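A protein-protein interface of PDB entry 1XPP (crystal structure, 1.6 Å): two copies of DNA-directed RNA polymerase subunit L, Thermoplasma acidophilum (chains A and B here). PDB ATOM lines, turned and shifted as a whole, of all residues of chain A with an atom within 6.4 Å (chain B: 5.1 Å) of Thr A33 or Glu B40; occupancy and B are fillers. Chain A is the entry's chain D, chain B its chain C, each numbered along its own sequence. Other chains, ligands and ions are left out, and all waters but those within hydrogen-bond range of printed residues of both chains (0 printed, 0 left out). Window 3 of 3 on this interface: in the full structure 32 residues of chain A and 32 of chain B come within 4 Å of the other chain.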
ATOM      1  N   TYR A  30      10.892  22.897  25.114  1.00  0.00           N
ATOM      2  CA  TYR A  30      11.127  22.716  23.708  1.00  0.00           C
ATOM      3  C   TYR A  30      10.842  21.282  23.364  1.00  0.00           C
ATOM      4  O   TYR A  30      10.915  20.399  24.232  1.00  0.00           O
ATOM      5  CB  TYR A  30      12.569  23.052  23.312  1.00  0.00           C
ATOM      6  CG  TYR A  30      12.864  24.515  23.412  1.00  0.00           C
ATOM      7  CD1 TYR A  30      13.343  25.048  24.596  1.00  0.00           C
ATOM      8  CD2 TYR A  30      12.600  25.365  22.338  1.00  0.00           C
ATOM      9  CE1 TYR A  30      13.604  26.403  24.719  1.00  0.00           C
ATOM     10  CE2 TYR A  30      12.874  26.740  22.436  1.00  0.00           C
ATOM     11  CZ  TYR A  30      13.361  27.235  23.648  1.00  0.00           C
ATOM     12  OH  TYR A  30      13.602  28.585  23.764  1.00  0.00           O
ATOM     13  N   ASP A  31      10.520  21.063  22.098  1.00  0.00           N
ATOM     14  CA  ASP A  31      10.487  19.713  21.554  1.00  0.00           C
ATOM     15  C   ASP A  31      11.900  19.147  21.642  1.00  0.00           C
ATOM     16  O   ASP A  31      12.848  19.846  21.300  1.00  0.00           O
ATOM     17  CB  ASP A  31       9.996  19.725  20.090  1.00  0.00           C
ATOM     18  CG  ASP A  31       8.539  19.324  19.976  1.00  0.00           C
ATOM     19  OD1 ASP A  31       7.683  20.170  20.266  1.00  0.00           O
ATOM     20  OD2 ASP A  31       8.247  18.154  19.613  1.00  0.00           O
ATOM     21  N   ASN A  32      12.045  17.925  22.172  1.00  0.00           N
ATOM     22  CA  ASN A  32      13.354  17.242  22.184  1.00  0.00           C
ATOM     23  C   ASN A  32      14.041  17.205  20.813  1.00  0.00           C
ATOM     24  O   ASN A  32      15.259  17.308  20.733  1.00  0.00           O
ATOM     25  CB  ASN A  32      13.265  15.808  22.759  1.00  0.00           C
ATOM     26  CG  ASN A  32      12.911  15.764  24.246  1.00  0.00           C
ATOM     27  OD1 ASN A  32      12.494  14.716  24.759  1.00  0.00           O
ATOM     28  ND2 ASN A  32      13.112  16.855  24.942  1.00  0.00           N
ATOM     29  N   THR A  33      13.249  17.060  19.739  1.00  0.00           N
ATOM     30  CA  THR A  33      13.805  17.099  18.393  1.00  0.00           C
ATOM     31  C   THR A  33      14.550  18.385  18.097  1.00  0.00           C
ATOM     32  O   THR A  33      15.637  18.354  17.483  1.00  0.00           O
ATOM     33  CB  THR A  33      12.732  16.806  17.333  1.00  0.00           C
ATOM     34  OG1 THR A  33      12.350  15.438  17.532  1.00  0.00           O
ATOM     35  CG2 THR A  33      13.321  16.903  15.914  1.00  0.00           C
ATOM     36  N   LEU A  34      13.977  19.505  18.537  1.00  0.00           N
ATOM     37  CA  LEU A  34      14.674  20.801  18.382  1.00  0.00           C
ATOM     38  C   LEU A  34      16.062  20.794  19.051  1.00  0.00           C
ATOM     39  O   LEU A  34      17.057  21.214  18.460  1.00  0.00           O
ATOM     40  CB  LEU A  34      13.817  21.975  18.915  1.00  0.00           C
ATOM     41  CG  LEU A  34      14.534  23.340  18.745  1.00  0.00           C
ATOM     42  CD1 LEU A  34      13.585  24.470  18.377  1.00  0.00           C
ATOM     43  CD2 LEU A  34      15.253  23.673  20.004  1.00  0.00           C
ATOM     44  N   LEU A  35      16.141  20.279  20.272  1.00  0.00           N
ATOM     45  CA  LEU A  35      17.417  20.312  20.965  1.00  0.00           C
ATOM     46  C   LEU A  35      18.465  19.475  20.247  1.00  0.00           C
ATOM     47  O   LEU A  35      19.616  19.887  20.124  1.00  0.00           O
ATOM     48  CB  LEU A  35      17.257  19.869  22.434  1.00  0.00           C
ATOM     49  CG  LEU A  35      16.117  20.588  23.217  1.00  0.00           C
ATOM     50  CD1 LEU A  35      16.003  20.047  24.637  1.00  0.00           C
ATOM     51  CD2 LEU A  35      16.329  22.048  23.267  1.00  0.00           C
ATOM     52  N   ARG A  36      18.073  18.275  19.810  1.00  0.00           N
ATOM     53  CA  ARG A  36      19.038  17.372  19.170  1.00  0.00           C
ATOM     54  C   ARG A  36      19.470  17.923  17.834  1.00  0.00           C
ATOM     55  O   ARG A  36      20.642  17.868  17.501  1.00  0.00           O
ATOM     56  CB  ARG A  36      18.427  15.979  19.021  1.00  0.00           C
ATOM     57  CG  ARG A  36      17.992  15.400  20.340  1.00  0.00           C
ATOM     58  CD  ARG A  36      17.752  13.911  20.211  1.00  0.00           C
ATOM     59  NE  ARG A  36      16.920  13.423  21.310  1.00  0.00           N
ATOM     60  CZ  ARG A  36      15.594  13.302  21.247  1.00  0.00           C
ATOM     61  NH1 ARG A  36      14.939  13.626  20.134  1.00  0.00           N
ATOM     62  NH2 ARG A  36      14.926  12.861  22.302  1.00  0.00           N
ATOM     63  N   THR A  37      18.519  18.507  17.092  1.00  0.00           N
ATOM     64  CA  THR A  37      18.824  19.120  15.785  1.00  0.00           C
ATOM     65  C   THR A  37      19.783  20.294  15.969  1.00  0.00           C
ATOM     66  O   THR A  37      20.748  20.455  15.232  1.00  0.00           O
ATOM     67  CB  THR A  37      17.541  19.596  15.065  1.00  0.00           C
ATOM     68  OG1 THR A  37      16.702  18.470  14.858  1.00  0.00           O
ATOM     69  CG2 THR A  37      17.852  20.227  13.692  1.00  0.00           C
ATOM     70  N   LEU A  38      19.531  21.080  17.004  1.00  0.00           N
ATOM     71  CA  LEU A  38      20.387  22.202  17.276  1.00  0.00           C
ATOM     72  C   LEU A  38      21.830  21.770  17.548  1.00  0.00           C
ATOM     73  O   LEU A  38      22.784  22.340  17.018  1.00  0.00           O
ATOM     74  CB  LEU A  38      19.812  23.007  18.436  1.00  0.00           C
ATOM     75  CG  LEU A  38      20.660  24.198  18.858  1.00  0.00           C
ATOM     76  CD1 LEU A  38      20.928  25.178  17.701  1.00  0.00           C
ATOM     77  CD2 LEU A  38      20.017  24.897  20.045  1.00  0.00           C
ATOM     78  N   ILE A  55      19.094  15.538  28.105  1.00  0.00           N
ATOM     79  CA  ILE A  55      17.654  15.521  28.175  1.00  0.00           C
ATOM     80  C   ILE A  55      17.224  14.469  29.171  1.00  0.00           C
ATOM     81  O   ILE A  55      16.620  14.801  30.202  1.00  0.00           O
ATOM     82  CB  ILE A  55      17.035  15.289  26.798  1.00  0.00           C
ATOM     83  CG1 ILE A  55      17.344  16.473  25.893  1.00  0.00           C
ATOM     84  CG2 ILE A  55      15.519  15.094  26.916  1.00  0.00           C
ATOM     85  CD1 ILE A  55      17.100  16.223  24.406  1.00  0.00           C
ATOM     86  N   ARG B  36      13.587  14.178   8.157  1.00  0.00           N
ATOM     87  CA  ARG B  36      12.917  13.456   9.213  1.00  0.00           C
ATOM     88  C   ARG B  36      12.080  14.448   9.993  1.00  0.00           C
ATOM     89  O   ARG B  36      10.918  14.219  10.288  1.00  0.00           O
ATOM     90  CB  ARG B  36      13.934  12.784  10.129  1.00  0.00           C
ATOM     91  CG  ARG B  36      13.314  11.866  11.145  1.00  0.00           C
ATOM     92  CD  ARG B  36      14.416  11.028  11.793  1.00  0.00           C
ATOM     93  NE  ARG B  36      15.605  10.992  10.940  1.00  0.00           N
ATOM     94  CZ  ARG B  36      16.613  10.136  11.075  1.00  0.00           C
ATOM     95  NH1 ARG B  36      16.601   9.207  12.039  1.00  0.00           N
ATOM     96  NH2 ARG B  36      17.633  10.199  10.237  1.00  0.00           N
ATOM     97  N   THR B  37      12.660  15.603  10.266  1.00  0.00           N
ATOM     98  CA  THR B  37      11.908  16.628  10.972  1.00  0.00           C
ATOM     99  C   THR B  37      10.676  17.128  10.221  1.00  0.00           C
ATOM    100  O   THR B  37       9.653  17.397  10.832  1.00  0.00           O
ATOM    101  CB  THR B  37      12.791  17.796  11.401  1.00  0.00           C
ATOM    102  OG1 THR B  37      13.296  18.504  10.253  1.00  0.00           O
ATOM    103  CG2 THR B  37      13.931  17.280  12.230  1.00  0.00           C
ATOM    104  N   LEU B  38      10.780  17.210   8.902  1.00  0.00           N
ATOM    105  CA  LEU B  38       9.665  17.632   8.081  1.00  0.00           C
ATOM    106  C   LEU B  38       8.501  16.664   8.237  1.00  0.00           C
ATOM    107  O   LEU B  38       7.380  17.084   8.519  1.00  0.00           O
ATOM    108  CB  LEU B  38      10.089  17.749   6.629  1.00  0.00           C
ATOM    109  CG  LEU B  38       8.956  18.032   5.635  1.00  0.00           C
ATOM    110  CD1 LEU B  38       8.263  19.393   5.871  1.00  0.00           C
ATOM    111  CD2 LEU B  38       9.550  17.971   4.245  1.00  0.00           C
ATOM    112  N   VAL B  39       8.753  15.367   8.072  1.00  0.00           N
ATOM    113  CA  VAL B  39       7.635  14.436   8.217  1.00  0.00           C
ATOM    114  C   VAL B  39       7.100  14.360   9.632  1.00  0.00           C
ATOM    115  O   VAL B  39       5.887  14.314   9.807  1.00  0.00           O
ATOM    116  CB  VAL B  39       7.902  13.020   7.628  1.00  0.00           C
ATOM    117  CG1 VAL B  39       8.019  13.148   6.123  1.00  0.00           C
ATOM    118  CG2 VAL B  39       9.105  12.359   8.237  1.00  0.00           C
ATOM    119  N   GLU B  40       7.976  14.385  10.624  1.00  0.00           N
ATOM    120  CA  GLU B  40       7.536  14.412  12.020  1.00  0.00           C
ATOM    121  C   GLU B  40       6.603  15.603  12.272  1.00  0.00           C
ATOM    122  O   GLU B  40       5.613  15.472  12.983  1.00  0.00           O
ATOM    123  CB  GLU B  40       8.731  14.424  12.974  1.00  0.00           C
ATOM    124  CG  GLU B  40       9.581  13.154  12.926  1.00  0.00           C
ATOM    125  CD  GLU B  40      10.846  13.219  13.777  1.00  0.00           C
ATOM    126  OE1 GLU B  40      11.272  14.325  14.163  1.00  0.00           O
ATOM    127  OE2 GLU B  40      11.429  12.145  14.040  1.00  0.00           O
ATOM    128  N   GLU B  41       6.894  16.751  11.659  1.00  0.00           N
ATOM    129  CA  GLU B  41       6.070  17.940  11.861  1.00  0.00           C
ATOM    130  C   GLU B  41       4.730  17.784  11.176  1.00  0.00           C
ATOM    131  O   GLU B  41       3.684  18.088  11.758  1.00  0.00           O
ATOM    132  CB  GLU B  41       6.797  19.183  11.333  1.00  0.00           C
ATOM    133  CG  GLU B  41       6.090  20.526  11.664  1.00  0.00           C
ATOM    134  CD  GLU B  41       6.160  20.898  13.140  1.00  0.00           C
ATOM    135  OE1 GLU B  41       6.791  20.167  13.929  1.00  0.00           O
ATOM    136  OE2 GLU B  41       5.606  21.956  13.506  1.00  0.00           O
ATOM    137  N   ILE B  42       4.742  17.305   9.932  1.00  0.00           N
ATOM    138  CA  ILE B  42       3.500  17.019   9.219  1.00  0.00           C
ATOM    139  C   ILE B  42       2.604  16.036  10.026  1.00  0.00           C
ATOM    140  O   ILE B  42       1.374  16.185  10.053  1.00  0.00           O
ATOM    141  CB  ILE B  42       3.787  16.530   7.763  1.00  0.00           C
ATOM    142  CG1 ILE B  42       4.590  17.579   6.997  1.00  0.00           C
ATOM    143  CG2 ILE B  42       2.479  16.251   7.019  1.00  0.00           C
ATOM    144  CD1 ILE B  42       5.064  17.198   5.620  1.00  0.00           C
ATOM    145  N   LEU B  43       3.208  15.092  10.741  1.00  0.00           N
ATOM    146  CA  LEU B  43       2.432  14.064  11.444  1.00  0.00           C
ATOM    147  C   LEU B  43       1.732  14.609  12.704  1.00  0.00           C
ATOM    148  O   LEU B  43       0.897  13.920  13.321  1.00  0.00           O
ATOM    149  CB  LEU B  43       3.321  12.879  11.799  1.00  0.00           C
ATOM    150  CG  LEU B  43       3.741  11.952  10.656  1.00  0.00           C
ATOM    151  CD1 LEU B  43       4.664  10.844  11.191  1.00  0.00           C
ATOM    152  CD2 LEU B  43       2.549  11.376   9.905  1.00  0.00           C
ATOM    153  N   LYS B  44       2.081  15.836  13.081  1.00  0.00           N
ATOM    154  CA  LYS B  44       1.459  16.504  14.229  1.00  0.00           C
ATOM    155  C   LYS B  44       0.099  17.091  13.865  1.00  0.00           C
ATOM    156  O   LYS B  44      -0.696  17.419  14.744  1.00  0.00           O
ATOM    157  CB  LYS B  44       2.371  17.590  14.784  1.00  0.00           C
ATOM    158  CG  LYS B  44       3.593  17.089  15.544  1.00  0.00           C
ATOM    159  CD  LYS B  44       4.553  18.256  15.776  1.00  0.00           C
ATOM    160  CE  LYS B  44       5.838  17.836  16.468  1.00  0.00           C
ATOM    161  NZ  LYS B  44       6.591  19.074  16.830  1.00  0.00           N
ATOM    162  N   TYR B  89      12.462  28.084  14.591  1.00  0.00           N
ATOM    163  CA  TYR B  89      13.880  28.488  14.595  1.00  0.00           C
ATOM    164  C   TYR B  89      14.085  30.004  14.540  1.00  0.00           C
ATOM    165  O   TYR B  89      15.065  30.528  15.069  1.00  0.00           O
ATOM    166  CB  TYR B  89      14.660  27.765  13.517  1.00  0.00           C
ATOM    167  CG  TYR B  89      14.893  26.352  13.918  1.00  0.00           C
ATOM    168  CD1 TYR B  89      15.894  26.040  14.828  1.00  0.00           C
ATOM    169  CD2 TYR B  89      14.055  25.350  13.449  1.00  0.00           C
ATOM    170  CE1 TYR B  89      16.067  24.733  15.249  1.00  0.00           C
ATOM    171  CE2 TYR B  89      14.230  24.032  13.854  1.00  0.00           C
ATOM    172  CZ  TYR B  89      15.235  23.739  14.743  1.00  0.00           C
ATOM    173  OH  TYR B  89      15.410  22.441  15.144  1.00  0.00           O
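The side-chain carboxylate (OE1) of Glu B41 is in salt-bridge range of the side-chain amino group (NZ) of Lys B44 (3.1 Å). OG1 of Thr A37 lies within hydrogen-bond range of O of Thr A33 (2.8 Å).
3 positions are printed for both chains. Of the 5 pairs that touch across the chains among the printed residues, none has its exchanged pair printed and touching as well.
Of the 10 printed residues of chain A, 4 touch a printed residue of chain B. Hydrophobic or aromatic side chains of chain A that line the printed part of chain B: Leu A34. Hydrophobic or aromatic side chains of chain B that line the printed part of chain A: Tyr B89. Among the printed residues, 5 pairs touch across the chains.
Of the printed residues of chain B, Thr A33 touches Thr B37 and Glu B40. Of the printed residues of chain B, Leu A34 touches Tyr B89. Of the printed residues of chain B, Thr A37 touches Tyr B89 (3.6 Å). Leu A38 touches none of the printed residues of chain B. Printed residues of chain A within 4 Å of Glu B40: Thr A33. Of the printed residues of chain A, Tyr B89 touches Leu A34 and Thr A37. The nearest printed residue of chain A that does not touch Glu B40 is Thr A37 (6.9 Å).
OD2 of Asp A31 lies within salt-bridge range of NZ of Lys B44.
Thr A33 touches Thr B37. Thr A33 touches Glu B40. Leu A34 touches Tyr B89 (CA to OH, 3.7 Å). CB of Thr A37 touches OH of Tyr B89, 3.6 Å away.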
